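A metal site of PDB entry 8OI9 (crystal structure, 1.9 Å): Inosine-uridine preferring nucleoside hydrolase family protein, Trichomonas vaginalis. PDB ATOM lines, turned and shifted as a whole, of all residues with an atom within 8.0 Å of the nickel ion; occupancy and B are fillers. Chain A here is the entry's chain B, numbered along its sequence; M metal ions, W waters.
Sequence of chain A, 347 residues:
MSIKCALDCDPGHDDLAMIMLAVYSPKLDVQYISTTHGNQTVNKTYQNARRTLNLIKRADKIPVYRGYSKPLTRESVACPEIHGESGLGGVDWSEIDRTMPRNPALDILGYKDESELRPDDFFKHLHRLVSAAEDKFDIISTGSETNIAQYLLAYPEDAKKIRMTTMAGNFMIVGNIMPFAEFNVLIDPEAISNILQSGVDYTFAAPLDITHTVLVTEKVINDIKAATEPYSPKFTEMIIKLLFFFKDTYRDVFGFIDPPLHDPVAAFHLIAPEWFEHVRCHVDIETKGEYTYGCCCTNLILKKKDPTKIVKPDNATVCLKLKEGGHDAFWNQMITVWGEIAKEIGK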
ATOM      1  N   ASN A  39       5.220 -28.081 -12.757  1.00  0.00           N
ATOM      2  CA  ASN A  39       4.253 -27.193 -12.119  1.00  0.00           C
ATOM      3  C   ASN A  39       4.753 -25.752 -12.164  1.00  0.00           C
ATOM      4  O   ASN A  39       3.947 -24.826 -12.258  1.00  0.00           O
ATOM      5  CB  ASN A  39       4.022 -27.619 -10.669  1.00  0.00           C
ATOM      6  CG  ASN A  39       2.595 -27.426 -10.218  1.00  0.00           C
ATOM      7  OD1 ASN A  39       2.356 -26.843  -9.161  1.00  0.00           O
ATOM      8  ND2 ASN A  39       1.651 -27.923 -10.990  1.00  0.00           N
ATOM      9  N   GLN A  40       6.068 -25.570 -12.014  1.00  0.00           N
ATOM     10  CA  GLN A  40       6.702 -24.266 -12.161  1.00  0.00           C
ATOM     11  C   GLN A  40       7.626 -24.289 -13.370  1.00  0.00           C
ATOM     12  O   GLN A  40       7.957 -25.352 -13.891  1.00  0.00           O
ATOM     13  CB  GLN A  40       7.499 -23.887 -10.906  1.00  0.00           C
ATOM     14  CG  GLN A  40       6.662 -23.737  -9.633  1.00  0.00           C
ATOM     15  CD  GLN A  40       5.457 -22.847  -9.772  1.00  0.00           C
ATOM     16  OE1 GLN A  40       5.497 -21.756 -10.337  1.00  0.00           O
ATOM     17  NE2 GLN A  40       4.329 -23.328  -9.268  1.00  0.00           N
ATOM     18  N   VAL A  77       2.257 -26.515 -18.500  1.00  0.00           N
ATOM     19  CA  VAL A  77       1.209 -26.322 -17.500  1.00  0.00           C
ATOM     20  C   VAL A  77       1.764 -25.503 -16.331  1.00  0.00           C
ATOM     21  O   VAL A  77       1.120 -25.439 -15.280  1.00  0.00           O
ATOM     22  CB  VAL A  77       0.646 -27.671 -17.005  1.00  0.00           C
ATOM     23  CG1 VAL A  77      -0.030 -28.437 -18.129  1.00  0.00           C
ATOM     24  CG2 VAL A  77       1.709 -28.535 -16.313  1.00  0.00           C
ATOM     25  N   ALA A  78       2.927 -24.879 -16.527  1.00  0.00           N
ATOM     26  CA  ALA A  78       3.584 -24.131 -15.464  1.00  0.00           C
ATOM     27  C   ALA A  78       2.768 -22.888 -15.124  1.00  0.00           C
ATOM     28  O   ALA A  78       2.280 -22.193 -16.022  1.00  0.00           O
ATOM     29  CB  ALA A  78       4.985 -23.763 -15.888  1.00  0.00           C
ATOM     30  N   CYS A  79       2.627 -22.609 -13.826  1.00  0.00           N
ATOM     31  CA  CYS A  79       1.991 -21.377 -13.394  1.00  0.00           C
ATOM     32  C   CYS A  79       2.740 -20.186 -13.990  1.00  0.00           C
ATOM     33  O   CYS A  79       3.943 -20.268 -14.230  1.00  0.00           O
ATOM     34  CB  CYS A  79       1.974 -21.240 -11.875  1.00  0.00           C
ATOM     35  SG  CYS A  79       0.967 -22.487 -11.030  1.00  0.00           S
ATOM     36  N   PRO A  80       2.048 -19.056 -14.282  1.00  0.00           N
ATOM     37  CA  PRO A  80       2.744 -17.818 -14.630  1.00  0.00           C
ATOM     38  C   PRO A  80       3.559 -17.352 -13.426  1.00  0.00           C
ATOM     39  O   PRO A  80       3.163 -17.602 -12.281  1.00  0.00           O
ATOM     40  CB  PRO A  80       1.626 -16.821 -14.996  1.00  0.00           C
ATOM     41  CG  PRO A  80       0.352 -17.427 -14.434  1.00  0.00           C
ATOM     42  CD  PRO A  80       0.584 -18.924 -14.311  1.00  0.00           C
ATOM     43  N   GLU A  81       4.692 -16.706 -13.678  1.00  0.00           N
ATOM     44  CA  GLU A  81       5.599 -16.314 -12.603  1.00  0.00           C
ATOM     45  C   GLU A  81       4.927 -15.262 -11.715  1.00  0.00           C
ATOM     46  O   GLU A  81       5.349 -15.072 -10.579  1.00  0.00           O
ATOM     47  CB  GLU A  81       6.937 -15.845 -13.168  1.00  0.00           C
ATOM     48  CG  GLU A  81       7.660 -16.934 -13.963  1.00  0.00           C
ATOM     49  CD  GLU A  81       9.171 -16.968 -13.829  1.00  0.00           C
ATOM     50  OE1 GLU A  81       9.725 -16.083 -13.131  1.00  0.00           O
ATOM     51  OE2 GLU A  81       9.798 -17.882 -14.399  1.00  0.00           O
ATOM     52  N   ILE A  82       3.850 -14.641 -12.216  1.00  0.00           N
ATOM     53  CA  ILE A  82       3.100 -13.633 -11.486  1.00  0.00           C
ATOM     54  C   ILE A  82       2.165 -14.264 -10.451  1.00  0.00           C
ATOM     55  O   ILE A  82       1.553 -13.562  -9.655  1.00  0.00           O
ATOM     56  CB  ILE A  82       2.356 -12.715 -12.495  1.00  0.00           C
ATOM     57  CG1 ILE A  82       3.345 -11.916 -13.331  1.00  0.00           C
ATOM     58  CG2 ILE A  82       1.348 -11.811 -11.795  1.00  0.00           C
ATOM     59  CD1 ILE A  82       2.738 -11.219 -14.530  1.00  0.00           C
ATOM     60  N   HIS A  83       2.063 -15.605 -10.412  1.00  0.00           N
ATOM     61  CA  HIS A  83       1.449 -16.279  -9.278  1.00  0.00           C
ATOM     62  C   HIS A  83       2.334 -16.185  -8.035  1.00  0.00           C
ATOM     63  O   HIS A  83       1.835 -16.305  -6.921  1.00  0.00           O
ATOM     64  CB  HIS A  83       1.151 -17.756  -9.575  1.00  0.00           C
ATOM     65  CG  HIS A  83      -0.091 -17.981 -10.372  1.00  0.00           C
ATOM     66  ND1 HIS A  83      -0.737 -19.199 -10.406  1.00  0.00           N
ATOM     67  CD2 HIS A  83      -0.834 -17.143 -11.110  1.00  0.00           C
ATOM     68  CE1 HIS A  83      -1.819 -19.099 -11.166  1.00  0.00           C
ATOM     69  NE2 HIS A  83      -1.893 -17.867 -11.606  1.00  0.00           N
ATOM     70  N   GLY A  84       3.650 -16.019  -8.238  1.00  0.00           N
ATOM     71  CA  GLY A  84       4.605 -15.916  -7.143  1.00  0.00           C
ATOM     72  C   GLY A  84       4.751 -17.226  -6.379  1.00  0.00           C
ATOM     73  O   GLY A  84       4.808 -17.224  -5.155  1.00  0.00           O
ATOM     74  N   GLU A  85       4.824 -18.342  -7.103  1.00  0.00           N
ATOM     75  CA  GLU A  85       5.019 -19.649  -6.500  1.00  0.00           C
ATOM     76  C   GLU A  85       6.444 -20.125  -6.766  1.00  0.00           C
ATOM     77  O   GLU A  85       6.841 -20.281  -7.928  1.00  0.00           O
ATOM     78  CB  GLU A  85       4.009 -20.662  -7.052  1.00  0.00           C
ATOM     79  CG  GLU A  85       2.568 -20.336  -6.686  1.00  0.00           C
ATOM     80  CD  GLU A  85       1.567 -21.327  -7.240  1.00  0.00           C
ATOM     81  OE1 GLU A  85       1.538 -22.478  -6.765  1.00  0.00           O
ATOM     82  OE2 GLU A  85       0.818 -20.945  -8.157  1.00  0.00           O
HETATM   83 NI    NI M   1      -0.249 -20.965  -9.747  1.00  0.00          NI
HETATM   84  O   HOH W   1      -1.546 -22.198  -9.035  1.00  0.00           O
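The backbone carbonyl oxygen (O) of Glu 85 sits close to the side-chain amide oxygen (OE1) of Gln 40, 3.1 Å away. N of Cys 79 lies within hydrogen-bond range of O of Asn 39 (3.0 Å).
Of the 11 residues printed, 3 come within 4 Å of the nickel ion. The nearest printed residue that does not touch the nickel ion is Pro 80 (5.1 Å).
The nickel ion is bound by the side-chain carboxylate (OE2) of Glu 85 (1.9 Å), water W1 (1.9 Å), a ring nitrogen (ND1) of His 83 (1.9 Å) and the side-chain sulfur (SG) of Cys 79 (2.3 Å). The nickel ion has four donor atoms within binding distance.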
